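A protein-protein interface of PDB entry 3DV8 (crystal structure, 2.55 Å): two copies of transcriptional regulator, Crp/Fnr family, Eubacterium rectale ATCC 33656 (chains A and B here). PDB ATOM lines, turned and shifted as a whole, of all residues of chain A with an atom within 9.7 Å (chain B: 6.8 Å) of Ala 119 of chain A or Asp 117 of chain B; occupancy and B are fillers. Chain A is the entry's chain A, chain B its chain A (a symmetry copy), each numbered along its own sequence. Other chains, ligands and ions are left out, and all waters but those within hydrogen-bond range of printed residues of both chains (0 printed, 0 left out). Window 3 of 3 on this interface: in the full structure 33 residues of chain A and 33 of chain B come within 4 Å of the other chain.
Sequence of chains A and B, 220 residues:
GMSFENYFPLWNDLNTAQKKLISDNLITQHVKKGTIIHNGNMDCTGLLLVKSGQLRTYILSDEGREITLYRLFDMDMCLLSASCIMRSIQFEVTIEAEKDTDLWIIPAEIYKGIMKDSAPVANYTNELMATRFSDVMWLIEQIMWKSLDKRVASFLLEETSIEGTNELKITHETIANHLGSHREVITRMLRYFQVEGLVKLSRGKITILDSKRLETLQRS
Asp 117 of chain B touches one residue of chain A.
Lys 116 of chain B touches just one residue of chain A: Ala 119 (3.2 Å).
Of chain A, only Ala 119 (3.9 Å) comes within 4 Å of Ser 118 of chain B.
Printed residues of chain B within 4 Å of Asn 126 of chain A: Ala 122.
Of the printed residues of chain B, Ser 118 of chain A touches Ala 119 (3.9 Å).
Of the printed residues of chain B, Ala 122 of chain A touches Ala 122 (3.4 Å) and Asn 123 (3.0 Å).
Of the printed residues of chain A, Ala 122 of chain B touches Ala 122, Asn 123 and Asn 126.
Printed residues of chain B within 4 Å of Asp 117 of chain A: Ala 119.
Glu 127 of chain A touches none of the printed residues of chain B.
The nearest printed residue of chain A that does not touch Met 115 of chain B is Ala 119 of chain A (4.1 Å).
O of Lys 116 of chain A touches CB of Ala 119 of chain B, at 3.2 Å.
Asp 117 of chain A touches Ala 119 of chain B.
Ser 118 of chain A touches Ala 119 of chain B.
Ala 119 of chain A touches Lys 116 of chain B (CB to O, 3.2 Å).
Ala 119 of chain A touches Asp 117 of chain B (CB to C, 3.8 Å).
C of Ser 118 of chain B touches CB of Ala 119 of chain A, 3.9 Å away.
N of Ala 119 of chain B touches CB of Ala 119 of chain A (3.8 Å).
Ala 122 of chain B touches Ala 122 of chain A (CB to CB, 3.4 Å).
Ala 122 of chain A touches Asn 123 of chain B (CB to OD1, 3.0 Å).
Ala 122 of chain B touches Asn 123 of chain A (CB to OD1, 3.0 Å).
Hydrophobic or aromatic side chains of chain B within 4 Å of the printed part of chain A: Ala 119 and Ala 122.
Among the printed residues, no Asp or Glu carboxylate lies within 4 Å of a Lys or Arg side-chain nitrogen of the other chain.
The backbone carbonyl oxygen (O) of Ala 119 of chain B lies close to the side-chain amide oxygen (OD1) of Asn 123 of chain B, 3.1 Å away.
The side-chain carboxylate (OD1) of Asp 117 of chain A is in salt-bridge range of the side-chain amino group (NZ) of Lys 116 of chain A.
The side-chain amide nitrogen (ND2) of Asn 126 of chain A lies within hydrogen-bond range of the backbone carbonyl oxygen (O) of Ala 122 of chain A, 3.0 Å away.
OD1 of Asn 123 of chain A sits close to O of Ala 119 of chain A (3.1 Å).
The side-chain amino group (NZ) of Lys 116 of chain B lies within salt-bridge range of the side-chain carboxylate (OD1) of Asp 117 of chain B, at 3.98 Å.
The backbone NH of Val 121 of chain A sits at hydrogen-bond distance from the side-chain hydroxyl of Ser 118 of chain A.
OD1 of Asn 123 of chain A lies close to O of Met 115 of chain B, 3.2 Å away.
O of Ala 122 of chain B lies within hydrogen-bond range of ND2 of Asn 126 of chain A (3.2 Å).
The side-chain amide oxygen of Asn 123 of chain B lies close to the backbone carbonyl oxygen of Met 115 of chain A (3.2 Å).
Met 115 of chain A touches Asn 123 of chain B, and with the chains exchanged Asn 123 of chain A touches Met 115 of chain B.
Lys 116 of chain A touches Ala 119 of chain B, and with the chains exchanged Ala 119 of chain A touches Lys 116 of chain B.
Ala 119 of chain A touches its own counterpart, Ala 119 of chain B.
Ala 122 of chain A touches its own counterpart, Ala 122 of chain B.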
ATOM      1  N   LEU A  10       6.398 -25.918   7.256  1.00  0.00           N
ATOM      2  CA  LEU A  10       7.147 -26.802   6.346  1.00  0.00           C
ATOM      3  C   LEU A  10       6.364 -28.087   5.957  1.00  0.00           C
ATOM      4  O   LEU A  10       6.715 -28.735   4.971  1.00  0.00           O
ATOM      5  CB  LEU A  10       8.477 -27.178   7.016  1.00  0.00           C
ATOM      6  CG  LEU A  10       9.534 -28.017   6.305  1.00  0.00           C
ATOM      7  CD1 LEU A  10       9.994 -27.368   4.996  1.00  0.00           C
ATOM      8  CD2 LEU A  10      10.696 -28.213   7.275  1.00  0.00           C
ATOM      9  N   ASP A  13       5.192 -28.654   2.406  1.00  0.00           N
ATOM     10  CA  ASP A  13       6.361 -28.880   1.551  1.00  0.00           C
ATOM     11  C   ASP A  13       6.958 -30.305   1.704  1.00  0.00           C
ATOM     12  O   ASP A  13       7.663 -30.759   0.797  1.00  0.00           O
ATOM     13  CB  ASP A  13       7.437 -27.806   1.809  1.00  0.00           C
ATOM     14  CG  ASP A  13       6.935 -26.379   1.532  1.00  0.00           C
ATOM     15  OD1 ASP A  13       6.346 -26.143   0.449  1.00  0.00           O
ATOM     16  OD2 ASP A  13       7.155 -25.490   2.396  1.00  0.00           O
ATOM     17  N   LEU A  14       6.682 -31.005   2.816  1.00  0.00           N
ATOM     18  CA  LEU A  14       7.186 -32.383   3.035  1.00  0.00           C
ATOM     19  C   LEU A  14       6.428 -33.427   2.208  1.00  0.00           C
ATOM     20  O   LEU A  14       5.246 -33.245   1.915  1.00  0.00           O
ATOM     21  CB  LEU A  14       7.088 -32.795   4.516  1.00  0.00           C
ATOM     22  CG  LEU A  14       7.876 -32.026   5.576  1.00  0.00           C
ATOM     23  CD1 LEU A  14       7.595 -32.644   6.936  1.00  0.00           C
ATOM     24  CD2 LEU A  14       9.374 -32.015   5.289  1.00  0.00           C
ATOM     25  N   ASN A  15       7.117 -34.518   1.849  1.00  0.00           N
ATOM     26  CA  ASN A  15       6.496 -35.664   1.137  1.00  0.00           C
ATOM     27  C   ASN A  15       5.866 -36.646   2.142  1.00  0.00           C
ATOM     28  O   ASN A  15       5.951 -36.419   3.347  1.00  0.00           O
ATOM     29  CB  ASN A  15       7.482 -36.346   0.158  1.00  0.00           C
ATOM     30  CG  ASN A  15       8.740 -36.923   0.825  1.00  0.00           C
ATOM     31  OD1 ASN A  15       8.724 -37.386   1.958  1.00  0.00           O
ATOM     32  ND2 ASN A  15       9.834 -36.918   0.085  1.00  0.00           N
ATOM     33  N   GLN A  18       8.588 -38.284   4.534  1.00  0.00           N
ATOM     34  CA  GLN A  18       9.052 -37.268   5.510  1.00  0.00           C
ATOM     35  C   GLN A  18       7.986 -36.930   6.556  1.00  0.00           C
ATOM     36  O   GLN A  18       8.303 -36.808   7.744  1.00  0.00           O
ATOM     37  CB  GLN A  18       9.478 -35.983   4.792  1.00  0.00           C
ATOM     38  CG  GLN A  18      10.760 -36.135   3.972  1.00  0.00           C
ATOM     39  CD  GLN A  18      10.952 -35.058   2.926  1.00  0.00           C
ATOM     40  OE1 GLN A  18      10.011 -34.370   2.526  1.00  0.00           O
ATOM     41  NE2 GLN A  18      12.185 -34.913   2.463  1.00  0.00           N
ATOM     42  N   TYR A 111      15.523 -35.172  12.108  1.00  0.00           N
ATOM     43  CA  TYR A 111      15.498 -33.887  11.396  1.00  0.00           C
ATOM     44  C   TYR A 111      16.757 -33.722  10.515  1.00  0.00           C
ATOM     45  O   TYR A 111      16.638 -33.332   9.349  1.00  0.00           O
ATOM     46  CB  TYR A 111      15.303 -32.709  12.366  1.00  0.00           C
ATOM     47  CG  TYR A 111      14.966 -31.424  11.649  1.00  0.00           C
ATOM     48  CD1 TYR A 111      13.644 -31.101  11.313  1.00  0.00           C
ATOM     49  CD2 TYR A 111      15.963 -30.547  11.281  1.00  0.00           C
ATOM     50  CE1 TYR A 111      13.331 -29.908  10.632  1.00  0.00           C
ATOM     51  CE2 TYR A 111      15.676 -29.351  10.592  1.00  0.00           C
ATOM     52  CZ  TYR A 111      14.357 -29.037  10.272  1.00  0.00           C
ATOM     53  OH  TYR A 111      14.073 -27.868   9.605  1.00  0.00           O
ATOM     54  N   GLY A 113      18.621 -36.132   9.232  1.00  0.00           N
ATOM     55  CA  GLY A 113      18.470 -37.086   8.121  1.00  0.00           C
ATOM     56  C   GLY A 113      17.655 -36.541   6.956  1.00  0.00           C
ATOM     57  O   GLY A 113      18.081 -36.657   5.816  1.00  0.00           O
ATOM     58  N   ILE A 114      16.493 -35.954   7.260  1.00  0.00           N
ATOM     59  CA  ILE A 114      15.599 -35.310   6.270  1.00  0.00           C
ATOM     60  C   ILE A 114      16.290 -34.109   5.595  1.00  0.00           C
ATOM     61  O   ILE A 114      16.148 -33.885   4.390  1.00  0.00           O
ATOM     62  CB  ILE A 114      14.254 -34.837   6.935  1.00  0.00           C
ATOM     63  CG1 ILE A 114      13.407 -36.043   7.375  1.00  0.00           C
ATOM     64  CG2 ILE A 114      13.415 -33.972   5.981  1.00  0.00           C
ATOM     65  CD1 ILE A 114      12.152 -35.684   8.144  1.00  0.00           C
ATOM     66  N   MET A 115      17.042 -33.365   6.400  1.00  0.00           N
ATOM     67  CA  MET A 115      17.784 -32.162   5.971  1.00  0.00           C
ATOM     68  C   MET A 115      18.913 -32.484   4.962  1.00  0.00           C
ATOM     69  O   MET A 115      19.185 -31.688   4.053  1.00  0.00           O
ATOM     70  CB  MET A 115      18.354 -31.482   7.218  1.00  0.00           C
ATOM     71  CG  MET A 115      18.614 -30.013   7.132  1.00  0.00           C
ATOM     72  SD  MET A 115      19.475 -29.354   8.779  1.00  0.00           S
ATOM     73  CE  MET A 115      18.912 -30.447   9.994  1.00  0.00           C
ATOM     74  N   LYS A 116      19.552 -33.645   5.138  1.00  0.00           N
ATOM     75  CA  LYS A 116      20.625 -34.130   4.257  1.00  0.00           C
ATOM     76  C   LYS A 116      20.142 -34.315   2.812  1.00  0.00           C
ATOM     77  O   LYS A 116      20.855 -33.949   1.887  1.00  0.00           O
ATOM     78  CB  LYS A 116      21.194 -35.456   4.815  1.00  0.00           C
ATOM     79  CG  LYS A 116      22.326 -36.157   4.025  1.00  0.00           C
ATOM     80  CD  LYS A 116      22.690 -37.493   4.718  1.00  0.00           C
ATOM     81  CE  LYS A 116      23.756 -38.301   3.975  1.00  0.00           C
ATOM     82  NZ  LYS A 116      23.321 -38.747   2.620  1.00  0.00           N
ATOM     83  N   ASP A 117      18.927 -34.845   2.644  1.00  0.00           N
ATOM     84  CA  ASP A 117      18.328 -35.139   1.323  1.00  0.00           C
ATOM     85  C   ASP A 117      17.370 -34.105   0.745  1.00  0.00           C
ATOM     86  O   ASP A 117      17.164 -34.110  -0.465  1.00  0.00           O
ATOM     87  CB  ASP A 117      17.556 -36.471   1.380  1.00  0.00           C
ATOM     88  CG  ASP A 117      18.438 -37.668   1.689  1.00  0.00           C
ATOM     89  OD1 ASP A 117      19.674 -37.608   1.502  1.00  0.00           O
ATOM     90  OD2 ASP A 117      17.871 -38.693   2.108  1.00  0.00           O
ATOM     91  N   SER A 118      16.766 -33.265   1.580  1.00  0.00           N
ATOM     92  CA  SER A 118      15.779 -32.273   1.137  1.00  0.00           C
ATOM     93  C   SER A 118      16.329 -30.838   1.094  1.00  0.00           C
ATOM     94  O   SER A 118      16.703 -30.273   2.135  1.00  0.00           O
ATOM     95  CB  SER A 118      14.559 -32.326   2.065  1.00  0.00           C
ATOM     96  OG  SER A 118      13.535 -31.417   1.690  1.00  0.00           O
ATOM     97  N   ALA A 119      16.386 -30.269  -0.112  1.00  0.00           N
ATOM     98  CA  ALA A 119      16.728 -28.859  -0.300  1.00  0.00           C
ATOM     99  C   ALA A 119      15.682 -27.959   0.400  1.00  0.00           C
ATOM    100  O   ALA A 119      16.085 -27.013   1.068  1.00  0.00           O
ATOM    101  CB  ALA A 119      16.859 -28.497  -1.788  1.00  0.00           C
ATOM    102  N   PRO A 120      14.352 -28.225   0.219  1.00  0.00           N
ATOM    103  CA  PRO A 120      13.292 -27.472   0.934  1.00  0.00           C
ATOM    104  C   PRO A 120      13.445 -27.392   2.454  1.00  0.00           C
ATOM    105  O   PRO A 120      13.297 -26.305   3.015  1.00  0.00           O
ATOM    106  CB  PRO A 120      12.016 -28.241   0.576  1.00  0.00           C
ATOM    107  CG  PRO A 120      12.291 -28.798  -0.749  1.00  0.00           C
ATOM    108  CD  PRO A 120      13.745 -29.152  -0.767  1.00  0.00           C
ATOM    109  N   VAL A 121      13.727 -28.532   3.096  1.00  0.00           N
ATOM    110  CA  VAL A 121      13.964 -28.597   4.550  1.00  0.00           C
ATOM    111  C   VAL A 121      15.305 -27.927   4.905  1.00  0.00           C
ATOM    112  O   VAL A 121      15.406 -27.267   5.952  1.00  0.00           O
ATOM    113  CB  VAL A 121      13.889 -30.067   5.108  1.00  0.00           C
ATOM    114  CG1 VAL A 121      14.272 -30.144   6.581  1.00  0.00           C
ATOM    115  CG2 VAL A 121      12.490 -30.650   4.906  1.00  0.00           C
ATOM    116  N   ALA A 122      16.320 -28.107   4.052  1.00  0.00           N
ATOM    117  CA  ALA A 122      17.633 -27.455   4.226  1.00  0.00           C
ATOM    118  C   ALA A 122      17.509 -25.926   4.163  1.00  0.00           C
ATOM    119  O   ALA A 122      18.023 -25.229   5.039  1.00  0.00           O
ATOM    120  CB  ALA A 122      18.601 -27.929   3.182  1.00  0.00           C
ATOM    121  N   ASN A 123      16.835 -25.430   3.124  1.00  0.00           N
ATOM    122  CA  ASN A 123      16.567 -23.991   2.951  1.00  0.00           C
ATOM    123  C   ASN A 123      15.653 -23.429   4.038  1.00  0.00           C
ATOM    124  O   ASN A 123      15.812 -22.285   4.437  1.00  0.00           O
ATOM    125  CB  ASN A 123      15.982 -23.659   1.559  1.00  0.00           C
ATOM    126  CG  ASN A 123      17.023 -23.732   0.441  1.00  0.00           C
ATOM    127  OD1 ASN A 123      17.936 -24.549   0.471  1.00  0.00           O
ATOM    128  ND2 ASN A 123      16.872 -22.872  -0.560  1.00  0.00           N
ATOM    129  N   TYR A 124      14.691 -24.224   4.501  1.00  0.00           N
ATOM    130  CA  TYR A 124      13.825 -23.792   5.592  1.00  0.00           C
ATOM    131  C   TYR A 124      14.650 -23.572   6.889  1.00  0.00           C
ATOM    132  O   TYR A 124      14.419 -22.598   7.610  1.00  0.00           O
ATOM    133  CB  TYR A 124      12.667 -24.774   5.817  1.00  0.00           C
ATOM    134  CG  TYR A 124      11.734 -24.278   6.891  1.00  0.00           C
ATOM    135  CD1 TYR A 124      10.772 -23.289   6.600  1.00  0.00           C
ATOM    136  CD2 TYR A 124      11.840 -24.748   8.211  1.00  0.00           C
ATOM    137  CE1 TYR A 124       9.922 -22.795   7.597  1.00  0.00           C
ATOM    138  CE2 TYR A 124      11.004 -24.262   9.208  1.00  0.00           C
ATOM    139  CZ  TYR A 124      10.045 -23.288   8.892  1.00  0.00           C
ATOM    140  OH  TYR A 124       9.220 -22.815   9.879  1.00  0.00           O
ATOM    141  N   THR A 125      15.597 -24.473   7.161  1.00  0.00           N
ATOM    142  CA  THR A 125      16.474 -24.351   8.328  1.00  0.00           C
ATOM    143  C   THR A 125      17.370 -23.098   8.230  1.00  0.00           C
ATOM    144  O   THR A 125      17.656 -22.483   9.265  1.00  0.00           O
ATOM    145  CB  THR A 125      17.297 -25.635   8.565  1.00  0.00           C
ATOM    146  OG1 THR A 125      16.415 -26.763   8.596  1.00  0.00           O
ATOM    147  CG2 THR A 125      18.047 -25.572   9.877  1.00  0.00           C
ATOM    148  N   ASN A 126      17.793 -22.731   7.008  1.00  0.00           N
ATOM    149  CA  ASN A 126      18.542 -21.472   6.745  1.00  0.00           C
ATOM    150  C   ASN A 126      17.730 -20.267   7.157  1.00  0.00           C
ATOM    151  O   ASN A 126      18.230 -19.394   7.865  1.00  0.00           O
ATOM    152  CB  ASN A 126      18.900 -21.285   5.253  1.00  0.00           C
ATOM    153  CG  ASN A 126      20.105 -22.079   4.834  1.00  0.00           C
ATOM    154  OD1 ASN A 126      21.221 -21.755   5.226  1.00  0.00           O
ATOM    155  ND2 ASN A 126      19.906 -23.097   3.999  1.00  0.00           N
ATOM    156  N   GLU A 127      16.478 -20.236   6.691  1.00  0.00           N
ATOM    157  CA  GLU A 127      15.536 -19.153   7.013  1.00  0.00           C
ATOM    158  C   GLU A 127      15.259 -19.068   8.520  1.00  0.00           C
ATOM    159  O   GLU A 127      15.096 -17.974   9.058  1.00  0.00           O
ATOM    160  CB  GLU A 127      14.223 -19.268   6.209  1.00  0.00           C
ATOM    161  CG  GLU A 127      14.369 -19.215   4.653  1.00  0.00           C
ATOM    162  CD  GLU A 127      15.128 -17.990   4.084  1.00  0.00           C
ATOM    163  OE1 GLU A 127      15.129 -16.912   4.722  1.00  0.00           O
ATOM    164  OE2 GLU A 127      15.707 -18.111   2.966  1.00  0.00           O
ATOM    165  N   GLN B  18      26.049 -27.802 -12.377  1.00  0.00           N
ATOM    166  CA  GLN B  18      26.323 -26.787 -11.331  1.00  0.00           C
ATOM    167  C   GLN B  18      27.728 -26.190 -11.447  1.00  0.00           C
ATOM    168  O   GLN B  18      27.897 -24.975 -11.304  1.00  0.00           O
ATOM    169  CB  GLN B  18      26.145 -27.388  -9.933  1.00  0.00           C
ATOM    170  CG  GLN B  18      24.691 -27.709  -9.584  1.00  0.00           C
ATOM    171  CD  GLN B  18      24.536 -28.687  -8.438  1.00  0.00           C
ATOM    172  OE1 GLN B  18      25.458 -29.423  -8.087  1.00  0.00           O
ATOM    173  NE2 GLN B  18      23.348 -28.706  -7.851  1.00  0.00           N
ATOM    174  N   LYS B 112      21.549 -18.707  -5.674  1.00  0.00           N
ATOM    175  CA  LYS B 112      20.161 -18.916  -5.186  1.00  0.00           C
ATOM    176  C   LYS B 112      19.462 -20.064  -5.924  1.00  0.00           C
ATOM    177  O   LYS B 112      18.812 -20.893  -5.289  1.00  0.00           O
ATOM    178  CB  LYS B 112      19.328 -17.632  -5.356  1.00  0.00           C
ATOM    179  CG  LYS B 112      17.957 -17.640  -4.681  1.00  0.00           C
ATOM    180  CD  LYS B 112      17.160 -16.424  -5.093  1.00  0.00           C
ATOM    181  CE  LYS B 112      15.835 -16.379  -4.371  1.00  0.00           C
ATOM    182  NZ  LYS B 112      14.918 -15.395  -5.015  1.00  0.00           N
ATOM    183  N   GLY B 113      19.601 -20.085  -7.255  1.00  0.00           N
ATOM    184  CA  GLY B 113      19.028 -21.124  -8.127  1.00  0.00           C
ATOM    185  C   GLY B 113      19.532 -22.526  -7.816  1.00  0.00           C
ATOM    186  O   GLY B 113      18.731 -23.443  -7.703  1.00  0.00           O
ATOM    187  N   ILE B 114      20.853 -22.673  -7.681  1.00  0.00           N
ATOM    188  CA  ILE B 114      21.520 -23.944  -7.316  1.00  0.00           C
ATOM    189  C   ILE B 114      21.095 -24.409  -5.909  1.00  0.00           C
ATOM    190  O   ILE B 114      20.886 -25.601  -5.666  1.00  0.00           O
ATOM    191  CB  ILE B 114      23.086 -23.809  -7.375  1.00  0.00           C
ATOM    192  CG1 ILE B 114      23.565 -23.617  -8.823  1.00  0.00           C
ATOM    193  CG2 ILE B 114      23.791 -25.040  -6.786  1.00  0.00           C
ATOM    194  CD1 ILE B 114      25.048 -23.345  -8.966  1.00  0.00           C
ATOM    195  N   MET B 115      20.967 -23.440  -5.009  1.00  0.00           N
ATOM    196  CA  MET B 115      20.583 -23.657  -3.599  1.00  0.00           C
ATOM    197  C   MET B 115      19.140 -24.199  -3.449  1.00  0.00           C
ATOM    198  O   MET B 115      18.865 -25.004  -2.549  1.00  0.00           O
ATOM    199  CB  MET B 115      20.741 -22.332  -2.850  1.00  0.00           C
ATOM    200  CG  MET B 115      20.987 -22.408  -1.379  1.00  0.00           C
ATOM    201  SD  MET B 115      21.019 -20.606  -0.577  1.00  0.00           S
ATOM    202  CE  MET B 115      21.552 -19.597  -1.876  1.00  0.00           C
ATOM    203  N   LYS B 116      18.243 -23.748  -4.331  1.00  0.00           N
ATOM    204  CA  LYS B 116      16.837 -24.180  -4.362  1.00  0.00           C
ATOM    205  C   LYS B 116      16.704 -25.689  -4.603  1.00  0.00           C
ATOM    206  O   LYS B 116      15.890 -26.334  -3.955  1.00  0.00           O
ATOM    207  CB  LYS B 116      16.075 -23.386  -5.449  1.00  0.00           C
ATOM    208  CG  LYS B 116      14.574 -23.698  -5.667  1.00  0.00           C
ATOM    209  CD  LYS B 116      14.035 -22.847  -6.843  1.00  0.00           C
ATOM    210  CE  LYS B 116      12.571 -23.132  -7.188  1.00  0.00           C
ATOM    211  NZ  LYS B 116      12.338 -24.527  -7.663  1.00  0.00           N
ATOM    212  N   ASP B 117      17.529 -26.233  -5.503  1.00  0.00           N
ATOM    213  CA  ASP B 117      17.503 -27.659  -5.894  1.00  0.00           C
ATOM    214  C   ASP B 117      18.500 -28.589  -5.212  1.00  0.00           C
ATOM    215  O   ASP B 117      18.266 -29.794  -5.206  1.00  0.00           O
ATOM    216  CB  ASP B 117      17.743 -27.794  -7.410  1.00  0.00           C
ATOM    217  CG  ASP B 117      16.666 -27.134  -8.253  1.00  0.00           C
ATOM    218  OD1 ASP B 117      15.541 -26.889  -7.763  1.00  0.00           O
ATOM    219  OD2 ASP B 117      16.953 -26.876  -9.435  1.00  0.00           O
ATOM    220  N   SER B 118      19.600 -28.061  -4.686  1.00  0.00           N
ATOM    221  CA  SER B 118      20.653 -28.871  -4.062  1.00  0.00           C
ATOM    222  C   SER B 118      20.648 -28.806  -2.526  1.00  0.00           C
ATOM    223  O   SER B 118      20.869 -27.734  -1.938  1.00  0.00           O
ATOM    224  CB  SER B 118      22.020 -28.415  -4.590  1.00  0.00           C
ATOM    225  OG  SER B 118      23.099 -29.170  -4.061  1.00  0.00           O
ATOM    226  N   ALA B 119      20.382 -29.950  -1.892  1.00  0.00           N
ATOM    227  CA  ALA B 119      20.502 -30.090  -0.441  1.00  0.00           C
ATOM    228  C   ALA B 119      21.964 -29.843   0.000  1.00  0.00           C
ATOM    229  O   ALA B 119      22.162 -29.133   0.979  1.00  0.00           O
ATOM    230  CB  ALA B 119      20.005 -31.461   0.043  1.00  0.00           C
ATOM    231  N   PRO B 120      22.976 -30.453  -0.690  1.00  0.00           N
ATOM    232  CA  PRO B 120      24.406 -30.189  -0.393  1.00  0.00           C
ATOM    233  C   PRO B 120      24.817 -28.715  -0.368  1.00  0.00           C
ATOM    234  O   PRO B 120      25.510 -28.302   0.564  1.00  0.00           O
ATOM    235  CB  PRO B 120      25.137 -30.917  -1.525  1.00  0.00           C
ATOM    236  CG  PRO B 120      24.255 -32.033  -1.865  1.00  0.00           C
ATOM    237  CD  PRO B 120      22.854 -31.532  -1.700  1.00  0.00           C
ATOM    238  N   ALA B 122      22.599 -26.191  -0.166  1.00  0.00           N
ATOM    239  CA  ALA B 122      21.732 -25.616   0.881  1.00  0.00           C
ATOM    240  C   ALA B 122      22.343 -25.805   2.277  1.00  0.00           C
ATOM    241  O   ALA B 122      22.430 -24.848   3.047  1.00  0.00           O
ATOM    242  CB  ALA B 122      20.366 -26.236   0.836  1.00  0.00           C
ATOM    243  N   ASN B 123      22.749 -27.039   2.581  1.00  0.00           N
ATOM    244  CA  ASN B 123      23.417 -27.375   3.851  1.00  0.00           C
ATOM    245  C   ASN B 123      24.780 -26.701   3.994  1.00  0.00           C
ATOM    246  O   ASN B 123      25.168 -26.338   5.095  1.00  0.00           O
ATOM    247  CB  ASN B 123      23.569 -28.900   4.057  1.00  0.00           C
ATOM    248  CG  ASN B 123      22.252 -29.588   4.418  1.00  0.00           C
ATOM    249  OD1 ASN B 123      21.182 -29.201   3.961  1.00  0.00           O
ATOM    250  ND2 ASN B 123      22.337 -30.628   5.240  1.00  0.00           N
